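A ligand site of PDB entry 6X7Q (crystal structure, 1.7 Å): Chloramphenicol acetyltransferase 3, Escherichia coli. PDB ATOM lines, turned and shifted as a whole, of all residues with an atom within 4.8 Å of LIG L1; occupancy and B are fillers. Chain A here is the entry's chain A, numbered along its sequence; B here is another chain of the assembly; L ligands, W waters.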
ATOM      1  N   LYS A  42     -10.019  25.658 -16.960  1.00  0.00           N
ATOM      2  CA  LYS A  42     -10.884  24.856 -16.091  1.00  0.00           C
ATOM      3  C   LYS A  42     -12.005  25.759 -15.533  1.00  0.00           C
ATOM      4  O   LYS A  42     -13.174  25.354 -15.464  1.00  0.00           O
ATOM      5  CB  LYS A  42      -9.984  24.131 -15.091  1.00  0.00           C
ATOM      6  CG  LYS A  42     -10.621  23.150 -14.109  1.00  0.00           C
ATOM      7  CD  LYS A  42     -11.392  22.025 -14.743  1.00  0.00           C
ATOM      8  CE  LYS A  42     -10.700  21.450 -15.958  1.00  0.00           C
ATOM      9  NZ  LYS A  42     -11.225  20.116 -16.299  1.00  0.00           N
ATOM     10  N   LYS A  51     -17.014  19.662 -22.784  1.00  0.00           N
ATOM     11  CA  LYS A  51     -16.179  18.715 -22.047  1.00  0.00           C
ATOM     12  C   LYS A  51     -14.718  18.983 -22.380  1.00  0.00           C
ATOM     13  O   LYS A  51     -14.405  19.552 -23.423  1.00  0.00           O
ATOM     14  CB  LYS A  51     -16.588  17.288 -22.402  1.00  0.00           C
ATOM     15  CG  LYS A  51     -17.962  16.891 -21.888  1.00  0.00           C
ATOM     16  CD  LYS A  51     -18.640  15.889 -22.786  1.00  0.00           C
ATOM     17  CE  LYS A  51     -18.000  14.518 -22.789  1.00  0.00           C
ATOM     18  NZ  LYS A  51     -18.893  13.525 -23.434  1.00  0.00           N
ATOM     19  N   PHE A  52     -13.853  18.609 -21.448  1.00  0.00           N
ATOM     20  CA  PHE A  52     -12.447  18.962 -21.496  1.00  0.00           C
ATOM     21  C   PHE A  52     -11.785  18.447 -22.785  1.00  0.00           C
ATOM     22  O   PHE A  52     -11.073  19.192 -23.431  1.00  0.00           O
ATOM     23  CB  PHE A  52     -11.752  18.382 -20.270  1.00  0.00           C
ATOM     24  CG  PHE A  52     -10.280  18.692 -20.274  1.00  0.00           C
ATOM     25  CD1 PHE A  52      -9.830  19.983 -20.046  1.00  0.00           C
ATOM     26  CD2 PHE A  52      -9.353  17.704 -20.600  1.00  0.00           C
ATOM     27  CE1 PHE A  52      -8.462  20.259 -20.042  1.00  0.00           C
ATOM     28  CE2 PHE A  52      -8.009  17.999 -20.604  1.00  0.00           C
ATOM     29  CZ  PHE A  52      -7.573  19.279 -20.339  1.00  0.00           C
ATOM     30  N   TYR A  53     -11.962  17.168 -23.136  1.00  0.00           N
ATOM     31  CA  TYR A  53     -11.205  16.596 -24.267  1.00  0.00           C
ATOM     32  C   TYR A  53     -11.564  17.229 -25.612  1.00  0.00           C
ATOM     33  O   TYR A  53     -10.671  17.725 -26.350  1.00  0.00           O
ATOM     34  CB  TYR A  53     -11.385  15.091 -24.311  1.00  0.00           C
ATOM     35  CG  TYR A  53     -10.567  14.335 -25.342  1.00  0.00           C
ATOM     36  CD1 TYR A  53      -9.199  14.534 -25.480  1.00  0.00           C
ATOM     37  CD2 TYR A  53     -11.147  13.348 -26.123  1.00  0.00           C
ATOM     38  CE1 TYR A  53      -8.428  13.774 -26.327  1.00  0.00           C
ATOM     39  CE2 TYR A  53     -10.391  12.570 -26.978  1.00  0.00           C
ATOM     40  CZ  TYR A  53      -9.025  12.783 -27.081  1.00  0.00           C
ATOM     41  OH  TYR A  53      -8.276  11.983 -27.940  1.00  0.00           O
ATOM     42  N   PRO A  54     -12.869  17.346 -25.991  1.00  0.00           N
ATOM     43  CA  PRO A  54     -13.244  18.071 -27.197  1.00  0.00           C
ATOM     44  C   PRO A  54     -12.874  19.559 -27.220  1.00  0.00           C
ATOM     45  O   PRO A  54     -12.560  20.094 -28.267  1.00  0.00           O
ATOM     46  CB  PRO A  54     -14.764  17.888 -27.316  1.00  0.00           C
ATOM     47  CG  PRO A  54     -15.222  17.397 -25.965  1.00  0.00           C
ATOM     48  CD  PRO A  54     -14.031  16.684 -25.355  1.00  0.00           C
ATOM     49  N   THR A  90      -7.914  10.026 -30.634  1.00  0.00           N
ATOM     50  CA  THR A  90      -8.175   8.672 -30.192  1.00  0.00           C
ATOM     51  C   THR A  90      -9.250   8.640 -29.099  1.00  0.00           C
ATOM     52  O   THR A  90      -9.409   9.575 -28.331  1.00  0.00           O
ATOM     53  CB  THR A  90      -6.888   7.976 -29.734  1.00  0.00           C
ATOM     54  OG1 THR A  90      -6.254   8.753 -28.733  1.00  0.00           O
ATOM     55  CG2 THR A  90      -5.958   7.736 -30.903  1.00  0.00           C
ATOM     56  N   VAL A  91      -9.966   7.516 -29.040  1.00  0.00           N
ATOM     57  CA  VAL A  91     -11.012   7.282 -28.080  1.00  0.00           C
ATOM     58  C   VAL A  91     -10.794   5.891 -27.494  1.00  0.00           C
ATOM     59  O   VAL A  91     -10.263   5.020 -28.176  1.00  0.00           O
ATOM     60  CB  VAL A  91     -12.385   7.396 -28.770  1.00  0.00           C
ATOM     61  CG1 VAL A  91     -12.572   8.752 -29.436  1.00  0.00           C
ATOM     62  CG2 VAL A  91     -12.595   6.286 -29.771  1.00  0.00           C
ATOM     63  N   PHE A  92     -11.279   5.683 -26.273  1.00  0.00           N
ATOM     64  CA  PHE A  92     -11.042   4.464 -25.530  1.00  0.00           C
ATOM     65  C   PHE A  92     -12.336   3.667 -25.404  1.00  0.00           C
ATOM     66  O   PHE A  92     -13.390   4.271 -25.245  1.00  0.00           O
ATOM     67  CB  PHE A  92     -10.513   4.785 -24.125  1.00  0.00           C
ATOM     68  CG  PHE A  92      -9.962   3.599 -23.391  1.00  0.00           C
ATOM     69  CD1 PHE A  92      -8.891   2.871 -23.903  1.00  0.00           C
ATOM     70  CD2 PHE A  92     -10.514   3.165 -22.198  1.00  0.00           C
ATOM     71  CE1 PHE A  92      -8.374   1.783 -23.210  1.00  0.00           C
ATOM     72  CE2 PHE A  92      -9.958   2.109 -21.483  1.00  0.00           C
ATOM     73  CZ  PHE A  92      -8.912   1.391 -22.010  1.00  0.00           C
ATOM     74  N   PHE A  99      -8.289   1.050 -28.172  1.00  0.00           N
ATOM     75  CA  PHE A  99      -8.601   2.392 -28.651  1.00  0.00           C
ATOM     76  C   PHE A  99      -8.887   2.374 -30.150  1.00  0.00           C
ATOM     77  O   PHE A  99      -8.569   1.420 -30.886  1.00  0.00           O
ATOM     78  CB  PHE A  99      -7.477   3.386 -28.297  1.00  0.00           C
ATOM     79  CG  PHE A  99      -6.262   3.305 -29.184  1.00  0.00           C
ATOM     80  CD1 PHE A  99      -5.232   2.420 -28.888  1.00  0.00           C
ATOM     81  CD2 PHE A  99      -6.141   4.092 -30.331  1.00  0.00           C
ATOM     82  CE1 PHE A  99      -4.110   2.310 -29.699  1.00  0.00           C
ATOM     83  CE2 PHE A  99      -5.032   3.940 -31.148  1.00  0.00           C
ATOM     84  CZ  PHE A  99      -4.022   3.059 -30.838  1.00  0.00           C
ATOM     85  N   TYR A 117     -18.278  16.974 -33.500  1.00  0.00           N
ATOM     86  CA  TYR A 117     -17.610  16.017 -32.652  1.00  0.00           C
ATOM     87  C   TYR A 117     -18.612  15.030 -32.042  1.00  0.00           C
ATOM     88  O   TYR A 117     -18.392  13.820 -32.071  1.00  0.00           O
ATOM     89  CB  TYR A 117     -16.864  16.767 -31.545  1.00  0.00           C
ATOM     90  CG  TYR A 117     -16.301  15.899 -30.450  1.00  0.00           C
ATOM     91  CD1 TYR A 117     -15.030  15.338 -30.549  1.00  0.00           C
ATOM     92  CD2 TYR A 117     -17.033  15.646 -29.302  1.00  0.00           C
ATOM     93  CE1 TYR A 117     -14.521  14.540 -29.543  1.00  0.00           C
ATOM     94  CE2 TYR A 117     -16.539  14.847 -28.293  1.00  0.00           C
ATOM     95  CZ  TYR A 117     -15.269  14.310 -28.394  1.00  0.00           C
ATOM     96  OH  TYR A 117     -14.816  13.552 -27.369  1.00  0.00           O
ATOM     97  N   SER A 144      -3.827  12.522 -29.205  1.00  0.00           N
ATOM     98  CA  SER A 144      -4.139  11.448 -28.279  1.00  0.00           C
ATOM     99  C   SER A 144      -4.021  11.942 -26.844  1.00  0.00           C
ATOM    100  O   SER A 144      -3.313  12.916 -26.530  1.00  0.00           O
ATOM    101  CB  SER A 144      -3.253  10.225 -28.449  1.00  0.00           C
ATOM    102  OG  SER A 144      -3.703   9.418 -29.515  1.00  0.00           O
ATOM    103  N   ALA A 145      -4.727  11.239 -25.944  1.00  0.00           N
ATOM    104  CA  ALA A 145      -4.608  11.499 -24.513  1.00  0.00           C
ATOM    105  C   ALA A 145      -4.339  10.191 -23.782  1.00  0.00           C
ATOM    106  O   ALA A 145      -4.809   9.122 -24.195  1.00  0.00           O
ATOM    107  CB  ALA A 145      -5.849  12.167 -23.962  1.00  0.00           C
ATOM    108  N   LEU A 146      -3.594  10.295 -22.676  1.00  0.00           N
ATOM    109  CA  LEU A 146      -3.410   9.233 -21.705  1.00  0.00           C
ATOM    110  C   LEU A 146      -3.959   9.743 -20.382  1.00  0.00           C
ATOM    111  O   LEU A 146      -3.223  10.206 -19.531  1.00  0.00           O
ATOM    112  CB  LEU A 146      -1.947   8.807 -21.528  1.00  0.00           C
ATOM    113  CG  LEU A 146      -1.257   8.007 -22.646  1.00  0.00           C
ATOM    114  CD1 LEU A 146      -1.042   8.882 -23.850  1.00  0.00           C
ATOM    115  CD2 LEU A 146       0.071   7.446 -22.162  1.00  0.00           C
ATOM    116  N   PRO A 147      -5.285   9.685 -20.172  1.00  0.00           N
ATOM    117  CA  PRO A 147      -5.908  10.306 -19.001  1.00  0.00           C
ATOM    118  C   PRO A 147      -5.691   9.625 -17.659  1.00  0.00           C
ATOM    119  O   PRO A 147      -6.031  10.198 -16.610  1.00  0.00           O
ATOM    120  CB  PRO A 147      -7.394  10.327 -19.414  1.00  0.00           C
ATOM    121  CG  PRO A 147      -7.548   9.182 -20.345  1.00  0.00           C
ATOM    122  CD  PRO A 147      -6.253   9.079 -21.109  1.00  0.00           C
ATOM    123  N   TRP A 148      -5.062   8.441 -17.677  1.00  0.00           N
ATOM    124  CA  TRP A 148      -4.903   7.597 -16.503  1.00  0.00           C
ATOM    125  C   TRP A 148      -3.578   7.871 -15.787  1.00  0.00           C
ATOM    126  O   TRP A 148      -3.447   7.431 -14.674  1.00  0.00           O
ATOM    127  CB  TRP A 148      -4.969   6.096 -16.889  1.00  0.00           C
ATOM    128  CG  TRP A 148      -6.015   5.745 -17.887  1.00  0.00           C
ATOM    129  CD1 TRP A 148      -7.321   5.430 -17.665  1.00  0.00           C
ATOM    130  CD2 TRP A 148      -5.827   5.656 -19.321  1.00  0.00           C
ATOM    131  NE1 TRP A 148      -7.964   5.177 -18.843  1.00  0.00           N
ATOM    132  CE2 TRP A 148      -7.077   5.280 -19.879  1.00  0.00           C
ATOM    133  CE3 TRP A 148      -4.738   5.854 -20.168  1.00  0.00           C
ATOM    134  CZ2 TRP A 148      -7.255   5.106 -21.252  1.00  0.00           C
ATOM    135  CZ3 TRP A 148      -4.905   5.636 -21.529  1.00  0.00           C
ATOM    136  CH2 TRP A 148      -6.145   5.290 -22.061  1.00  0.00           C
ATOM    137  N   PHE A 154       7.054  12.597 -23.236  1.00  0.00           N
ATOM    138  CA  PHE A 154       6.491  11.573 -24.094  1.00  0.00           C
ATOM    139  C   PHE A 154       7.225  11.678 -25.439  1.00  0.00           C
ATOM    140  O   PHE A 154       7.418  12.797 -25.914  1.00  0.00           O
ATOM    141  CB  PHE A 154       4.977  11.724 -24.258  1.00  0.00           C
ATOM    142  CG  PHE A 154       4.306  10.656 -25.089  1.00  0.00           C
ATOM    143  CD1 PHE A 154       4.201  10.755 -26.473  1.00  0.00           C
ATOM    144  CD2 PHE A 154       3.796   9.528 -24.454  1.00  0.00           C
ATOM    145  CE1 PHE A 154       3.591   9.729 -27.188  1.00  0.00           C
ATOM    146  CE2 PHE A 154       3.190   8.513 -25.188  1.00  0.00           C
ATOM    147  CZ  PHE A 154       3.124   8.620 -26.550  1.00  0.00           C
ATOM    148  N   THR A 170       0.222  14.769 -27.978  1.00  0.00           N
ATOM    149  CA  THR A 170      -0.193  13.818 -26.953  1.00  0.00           C
ATOM    150  C   THR A 170      -0.315  14.540 -25.597  1.00  0.00           C
ATOM    151  O   THR A 170       0.635  15.182 -25.134  1.00  0.00           O
ATOM    152  CB  THR A 170       0.802  12.649 -26.805  1.00  0.00           C
ATOM    153  OG1 THR A 170       1.068  12.100 -28.113  1.00  0.00           O
ATOM    154  CG2 THR A 170       0.319  11.550 -25.877  1.00  0.00           C
ATOM    155  N   ALA A 172      -1.380  14.226 -21.298  1.00  0.00           N
ATOM    156  CA  ALA A 172      -1.417  13.326 -20.147  1.00  0.00           C
ATOM    157  C   ALA A 172      -2.506  13.786 -19.181  1.00  0.00           C
ATOM    158  O   ALA A 172      -3.151  14.819 -19.375  1.00  0.00           O
ATOM    159  CB  ALA A 172      -0.086  13.334 -19.422  1.00  0.00           C
ATOM    160  N   LYS A 173      -2.593  13.048 -18.078  1.00  0.00           N
ATOM    161  CA  LYS A 173      -3.454  13.428 -16.970  1.00  0.00           C
ATOM    162  C   LYS A 173      -2.954  14.744 -16.406  1.00  0.00           C
ATOM    163  O   LYS A 173      -1.788  14.849 -16.029  1.00  0.00           O
ATOM    164  CB  LYS A 173      -3.465  12.354 -15.883  1.00  0.00           C
ATOM    165  CG  LYS A 173      -4.357  12.659 -14.689  1.00  0.00           C
ATOM    166  CD  LYS A 173      -4.015  11.822 -13.488  1.00  0.00           C
ATOM    167  CE  LYS A 173      -4.762  10.527 -13.565  1.00  0.00           C
ATOM    168  NZ  LYS A 173      -4.517   9.629 -12.409  1.00  0.00           N
ATOM    169  N   TYR A 174      -3.854  15.736 -16.337  1.00  0.00           N
ATOM    170  CA  TYR A 174      -3.496  17.000 -15.694  1.00  0.00           C
ATOM    171  C   TYR A 174      -3.380  16.851 -14.173  1.00  0.00           C
ATOM    172  O   TYR A 174      -3.946  15.948 -13.554  1.00  0.00           O
ATOM    173  CB  TYR A 174      -4.416  18.148 -16.159  1.00  0.00           C
ATOM    174  CG  TYR A 174      -5.883  18.004 -15.873  1.00  0.00           C
ATOM    175  CD1 TYR A 174      -6.360  17.973 -14.558  1.00  0.00           C
ATOM    176  CD2 TYR A 174      -6.793  17.977 -16.914  1.00  0.00           C
ATOM    177  CE1 TYR A 174      -7.720  17.891 -14.306  1.00  0.00           C
ATOM    178  CE2 TYR A 174      -8.149  17.915 -16.675  1.00  0.00           C
ATOM    179  CZ  TYR A 174      -8.605  17.873 -15.364  1.00  0.00           C
ATOM    180  OH  TYR A 174      -9.965  17.749 -15.120  1.00  0.00           O
ATOM    181  N   LEU A 183      -1.403  20.762 -17.488  1.00  0.00           N
ATOM    182  CA  LEU A 183      -1.669  19.699 -18.464  1.00  0.00           C
ATOM    183  C   LEU A 183      -0.385  19.403 -19.221  1.00  0.00           C
ATOM    184  O   LEU A 183       0.136  20.265 -19.941  1.00  0.00           O
ATOM    185  CB  LEU A 183      -2.763  20.148 -19.456  1.00  0.00           C
ATOM    186  CG  LEU A 183      -3.072  19.200 -20.614  1.00  0.00           C
ATOM    187  CD1 LEU A 183      -3.760  17.941 -20.128  1.00  0.00           C
ATOM    188  CD2 LEU A 183      -3.879  19.888 -21.715  1.00  0.00           C
ATOM    189  N   PHE B  30       7.003   3.918 -27.973  1.00  0.00           N
ATOM    190  CA  PHE B  30       7.081   5.196 -27.324  1.00  0.00           C
ATOM    191  C   PHE B  30       7.737   5.054 -25.965  1.00  0.00           C
ATOM    192  O   PHE B  30       7.735   3.967 -25.372  1.00  0.00           O
ATOM    193  CB  PHE B  30       5.726   5.888 -27.218  1.00  0.00           C
ATOM    194  CG  PHE B  30       4.665   5.060 -26.496  1.00  0.00           C
ATOM    195  CD1 PHE B  30       3.927   4.108 -27.147  1.00  0.00           C
ATOM    196  CD2 PHE B  30       4.478   5.210 -25.125  1.00  0.00           C
ATOM    197  CE1 PHE B  30       2.986   3.341 -26.461  1.00  0.00           C
ATOM    198  CE2 PHE B  30       3.548   4.443 -24.458  1.00  0.00           C
ATOM    199  CZ  PHE B  30       2.798   3.535 -25.121  1.00  0.00           C
ATOM    200  N   HIS B 191       4.761  -0.237 -29.614  1.00  0.00           N
ATOM    201  CA  HIS B 191       3.322  -0.007 -29.742  1.00  0.00           C
ATOM    202  C   HIS B 191       2.582  -1.251 -30.264  1.00  0.00           C
ATOM    203  O   HIS B 191       1.353  -1.351 -30.167  1.00  0.00           O
ATOM    204  CB  HIS B 191       3.072   1.202 -30.641  1.00  0.00           C
ATOM    205  CG  HIS B 191       1.835   1.983 -30.291  1.00  0.00           C
ATOM    206  ND1 HIS B 191       0.667   1.426 -29.825  1.00  0.00           N
ATOM    207  CD2 HIS B 191       1.634   3.328 -30.367  1.00  0.00           C
ATOM    208  CE1 HIS B 191      -0.217   2.397 -29.629  1.00  0.00           C
ATOM    209  NE2 HIS B 191       0.362   3.595 -29.928  1.00  0.00           N
ATOM    210  N   ASP B 195      -0.264  -0.135 -25.732  1.00  0.00           N
ATOM    211  CA  ASP B 195      -0.831   1.184 -25.938  1.00  0.00           C
ATOM    212  C   ASP B 195      -0.608   2.038 -24.678  1.00  0.00           C
ATOM    213  O   ASP B 195      -0.093   1.572 -23.676  1.00  0.00           O
ATOM    214  CB  ASP B 195      -2.317   1.074 -26.255  1.00  0.00           C
ATOM    215  CG  ASP B 195      -2.683   0.095 -27.337  1.00  0.00           C
ATOM    216  OD1 ASP B 195      -1.950   0.066 -28.392  1.00  0.00           O
ATOM    217  OD2 ASP B 195      -3.716  -0.633 -27.142  1.00  0.00           O
ATOM    218  N   GLY B 196      -1.008   3.306 -24.763  1.00  0.00           N
ATOM    219  CA  GLY B 196      -0.877   4.218 -23.644  1.00  0.00           C
ATOM    220  C   GLY B 196      -1.588   3.672 -22.405  1.00  0.00           C
ATOM    221  O   GLY B 196      -1.069   3.800 -21.316  1.00  0.00           O
ATOM    222  N   PHE B 197      -2.736   3.008 -22.606  1.00  0.00           N
ATOM    223  CA  PHE B 197      -3.484   2.411 -21.511  1.00  0.00           C
ATOM    224  C   PHE B 197      -2.609   1.446 -20.709  1.00  0.00           C
ATOM    225  O   PHE B 197      -2.650   1.445 -19.488  1.00  0.00           O
ATOM    226  CB  PHE B 197      -4.758   1.698 -21.997  1.00  0.00           C
ATOM    227  CG  PHE B 197      -5.437   0.928 -20.915  1.00  0.00           C
ATOM    228  CD1 PHE B 197      -6.243   1.561 -19.972  1.00  0.00           C
ATOM    229  CD2 PHE B 197      -5.269  -0.455 -20.831  1.00  0.00           C
ATOM    230  CE1 PHE B 197      -6.872   0.827 -18.971  1.00  0.00           C
ATOM    231  CE2 PHE B 197      -5.872  -1.165 -19.795  1.00  0.00           C
ATOM    232  CZ  PHE B 197      -6.653  -0.532 -18.874  1.00  0.00           C
HETATM  233  N1  LIG L   1      -6.539  14.820 -17.189  1.00  0.00           N
HETATM  234  C1  LIG L   1      -7.408  14.746 -16.164  1.00  0.00           C
HETATM  235  N2  LIG L   1      -8.709  14.521 -16.353  1.00  0.00           N
HETATM  236  C2  LIG L   1      -9.216  14.357 -17.594  1.00  0.00           C
HETATM  237  C3  LIG L   1      -8.330  14.441 -18.770  1.00  0.00           C
HETATM  238  C4  LIG L   1      -6.932  14.706 -18.465  1.00  0.00           C
HETATM  239  N3  LIG L   1      -6.108  14.769 -19.505  1.00  0.00           N
HETATM  240  N4  LIG L   1      -9.070  14.250 -19.906  1.00  0.00           N
HETATM  241  C5  LIG L   1     -10.337  14.010 -19.484  1.00  0.00           C
HETATM  242  N5  LIG L   1     -10.450  14.150 -18.142  1.00  0.00           N
HETATM  243  C6  LIG L   1     -11.695  13.908 -17.377  1.00  0.00           C
HETATM  244  C7  LIG L   1     -12.838  14.879 -17.647  1.00  0.00           C
HETATM  245  O1  LIG L   1     -12.666  15.883 -16.681  1.00  0.00           O
HETATM  246  C8  LIG L   1     -14.031  13.963 -17.379  1.00  0.00           C
HETATM  247  O2  LIG L   1     -14.098  13.726 -15.945  1.00  0.00           O
HETATM  248  P1  LIG L   1     -15.287  14.460 -15.032  1.00  0.00           P
HETATM  249  O3  LIG L   1     -15.300  13.757 -13.650  1.00  0.00           O
HETATM  250  O4  LIG L   1     -14.837  15.936 -14.968  1.00  0.00           O
HETATM  251  O5  LIG L   1     -16.634  14.357 -15.754  1.00  0.00           O
HETATM  252  C9  LIG L   1     -13.619  12.606 -17.912  1.00  0.00           C
HETATM  253  O6  LIG L   1     -12.179  12.604 -17.809  1.00  0.00           O
HETATM  254  C10 LIG L   1     -14.106  12.276 -19.288  1.00  0.00           C
HETATM  255  O7  LIG L   1     -13.460  13.143 -20.200  1.00  0.00           O
HETATM  256  P2  LIG L   1     -14.276  14.228 -21.125  1.00  0.00           P
HETATM  257  O8  LIG L   1     -13.341  15.307 -21.553  1.00  0.00           O
HETATM  258  O9  LIG L   1     -15.479  14.874 -20.315  1.00  0.00           O
HETATM  259  O10 LIG L   1     -14.743  13.382 -22.467  1.00  0.00           O
HETATM  260  P3  LIG L   1     -14.626  11.821 -22.850  1.00  0.00           P
HETATM  261  O11 LIG L   1     -14.717  12.078 -24.358  1.00  0.00           O
HETATM  262  O12 LIG L   1     -15.648  10.839 -22.437  1.00  0.00           O
HETATM  263  O13 LIG L   1     -13.209  11.055 -22.692  1.00  0.00           O
HETATM  264  C11 LIG L   1     -10.877  10.703 -22.666  1.00  0.00           C
HETATM  265  C12 LIG L   1     -11.965  11.719 -22.977  1.00  0.00           C
HETATM  266  C13 LIG L   1     -11.055  10.202 -21.233  1.00  0.00           C
HETATM  267  C14 LIG L   1      -9.534  11.441 -22.814  1.00  0.00           C
HETATM  268  C15 LIG L   1     -11.029   9.505 -23.683  1.00  0.00           C
HETATM  269  O14 LIG L   1     -11.025   9.969 -25.096  1.00  0.00           O
HETATM  270  C16 LIG L   1      -9.845   8.556 -23.509  1.00  0.00           C
HETATM  271  O15 LIG L   1      -9.710   7.817 -22.578  1.00  0.00           O
HETATM  272  N6  LIG L   1      -8.958   8.597 -24.483  1.00  0.00           N
HETATM  273  C17 LIG L   1      -7.775   7.735 -24.543  1.00  0.00           C
HETATM  274  C18 LIG L   1      -7.792   6.963 -25.843  1.00  0.00           C
HETATM  275  C19 LIG L   1      -6.522   6.159 -25.968  1.00  0.00           C
HETATM  276  O16 LIG L   1      -6.333   5.110 -25.379  1.00  0.00           O
HETATM  277  N7  LIG L   1      -5.569   6.646 -26.774  1.00  0.00           N
HETATM  278  C20 LIG L   1      -4.319   5.922 -26.913  1.00  0.00           C
HETATM  279  C21 LIG L   1      -3.391   6.463 -25.847  1.00  0.00           C
HETATM  280  C22 LIG L   1      -0.965   6.677 -26.762  1.00  0.00           C
HETATM  281  O17 LIG L   1      -1.167   7.751 -27.333  1.00  0.00           O
HETATM  282  C23 LIG L   1       0.399   6.049 -26.668  1.00  0.00           C
HETATM  283  O18 LIG L   1      -2.093   5.898 -26.208  1.00  0.00           O
HETATM  284  C1  LG2 L   2      -2.734   7.283 -35.328  1.00  0.00           C
HETATM  285 CL1  LG2 L   2      -1.886   7.001 -36.897  1.00  0.00          CL
HETATM  286 CL2  LG2 L   2      -4.267   6.455 -35.300  1.00  0.00          CL
HETATM  287  C2  LG2 L   2      -1.921   6.651 -34.260  1.00  0.00           C
HETATM  288  O1  LG2 L   2      -1.278   5.682 -34.568  1.00  0.00           O
HETATM  289  N1  LG2 L   2      -1.955   7.123 -33.004  1.00  0.00           N
HETATM  290  C3  LG2 L   2      -1.037   6.652 -31.957  1.00  0.00           C
HETATM  291  C4  LG2 L   2      -1.790   6.336 -30.650  1.00  0.00           C
HETATM  292  O2  LG2 L   2      -0.915   5.887 -29.598  1.00  0.00           O
HETATM  293  C5  LG2 L   2       0.152   7.636 -31.766  1.00  0.00           C
HETATM  294  O3  LG2 L   2      -0.295   8.878 -31.214  1.00  0.00           O
HETATM  295  C6  LG2 L   2       0.898   7.879 -33.051  1.00  0.00           C
HETATM  296  C7  LG2 L   2       1.925   7.016 -33.436  1.00  0.00           C
HETATM  297  C8  LG2 L   2       2.619   7.230 -34.610  1.00  0.00           C
HETATM  298  C9  LG2 L   2       2.234   8.315 -35.408  1.00  0.00           C
HETATM  299  N2  LG2 L   2       2.974   8.595 -36.677  1.00  0.00           N
HETATM  300  O4  LG2 L   2       4.095   8.134 -36.827  1.00  0.00           O
HETATM  301  O5  LG2 L   2       2.391   9.271 -37.516  1.00  0.00           O
HETATM  302  C10 LG2 L   2       1.210   9.181 -35.047  1.00  0.00           C
HETATM  303  C11 LG2 L   2       0.554   8.958 -33.861  1.00  0.00           C
HETATM  304  O   HOH W   1     -13.589  16.936 -12.928  1.00  0.00           O
HETATM  305  O   HOH W   2      -4.564   3.010 -24.930  1.00  0.00           O
HETATM  306  O   HOH W   3     -15.143  16.980 -18.786  1.00  0.00           O
HETATM  307  O   HOH W   4     -15.289  18.368 -14.645  1.00  0.00           O
HETATM  308  O   HOH W   5     -15.589  11.266 -13.158  1.00  0.00           O
HETATM  309  O   HOH W   6      -8.258  11.579 -15.513  1.00  0.00           O
HETATM  310  O   HOH W   7     -13.407   7.694 -25.442  1.00  0.00           O
HETATM  311  O   HOH W   8     -17.702  12.442 -17.517  1.00  0.00           O
HETATM  312  O   HOH W   9       0.497   9.363 -28.866  1.00  0.00           O
HETATM  313  O   HOH W  10     -11.835   6.898 -21.337  1.00  0.00           O
HETATM  314  O   HOH W  11     -16.657  14.416 -11.307  1.00  0.00           O
HETATM  315  O   HOH W  12      -7.378  14.470 -22.124  1.00  0.00           O
HETATM  316  O   HOH W  13     -12.608  13.148 -13.476  1.00  0.00           O
HETATM  317  O   HOH W  14     -13.420  10.297 -26.160  1.00  0.00           O
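O2 of LG2 L2 sits close to O17 of LIG L1 (2.9 Å).
The side-chain hydroxyl (OH) of Tyr 53 is in hydrogen-bond range of the backbone carbonyl oxygen (O) of Thr 90, 2.7 Å away. The side-chain hydroxyl of Tyr 174 sits at hydrogen-bond distance from the side-chain amino group of Lys 42, 2.9 Å away. The backbone carbonyl oxygen (O) of Trp 148 is in hydrogen-bond range of the side-chain amino group (NZ) of Lys 173 (3.3 Å). N of Lys 173 sits at hydrogen-bond distance from O of Leu 146 (3.3 Å). OG1 of Thr 90 is in hydrogen-bond range of OG of Ser 144 (2.7 Å).
Water W3 bridges O9 of LIG L1 (2.6 Å) and N of Phe 52 (3.4 Å). Water W9 lies within hydrogen-bond range of O3 of LG2 L2, O17 of LIG L1 and OG1 of Thr 170. Water W2 lies within hydrogen-bond range of O16 of LIG L1 (2.8 Å) and N of Phe 197 of chain B (3.0 Å). Water W6 bridges the backbone carbonyl oxygen of Pro 147 and a nitrogen (N2) of LIG L1. Water W7 lies within hydrogen-bond range of N of Phe 92 and O14 of LIG L1.
Residues that only touch LIG L1: Lys 51 (3.4 Å), Val 91 (3.6 Å), Phe 92 (3.5 Å), Phe 99 (3.6 Å), Ser 144 (3.4 Å), Ala 145 (3.3 Å), Leu 146 (3.7 Å), Pro 147 (3.4 Å), Trp 148 (3.3 Å), Phe 154 (3.7 Å), Lys 173 (3.4 Å), Leu 183 (3.995 Å) and Phe 30 of chain B (3.8 Å). Hydrophobic or aromatic side chains within 4 Å of LIG L1: Phe 52, Tyr 53, Phe 92, Phe 99, Ala 145, Leu 146, Pro 147, Trp 148, Phe 154, Tyr 174, Leu 183 and Phe 30 of chain B. Within 4 Å of LIG L1: Lys 51, Phe 52, Tyr 53, Thr 90, Val 91, Phe 92, Phe 99, Tyr 117, Ser 144, Ala 145, Leu 146, Pro 147, Trp 148, Phe 154, Ala 172, Lys 173, Tyr 174, Leu 183, Phe 30 of chain B and Gly 196 of chain B. The nearest printed residue that does not touch LIG L1 is His 191 of chain B (4.1 Å).
OG1 of Thr 90 sits at hydrogen-bond distance from N7 of LIG L1, 3.0 Å away. The backbone NH (N) of Phe 52 sits at hydrogen-bond distance from an oxygen (O8) of LIG L1. N of Tyr 53 lies within hydrogen-bond range of O8 of LIG L1, 2.8 Å away. OH of Tyr 117 lies within hydrogen-bond range of O11 of LIG L1, 3.4 Å away. A ring nitrogen (NE2) of His 191 of chain B sits at hydrogen-bond distance from an oxygen (O2) of LG2 L2 (2.6 Å). N of Tyr 174 is in hydrogen-bond range of N1 of LIG L1, at 3.0 Å. The backbone carbonyl oxygen (O) of Ala 172 sits at hydrogen-bond distance from a nitrogen (N3) of LIG L1 (3.0 Å). N of Gly 196 of chain B lies within hydrogen-bond range of O18 of LIG L1, 3.2 Å away.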
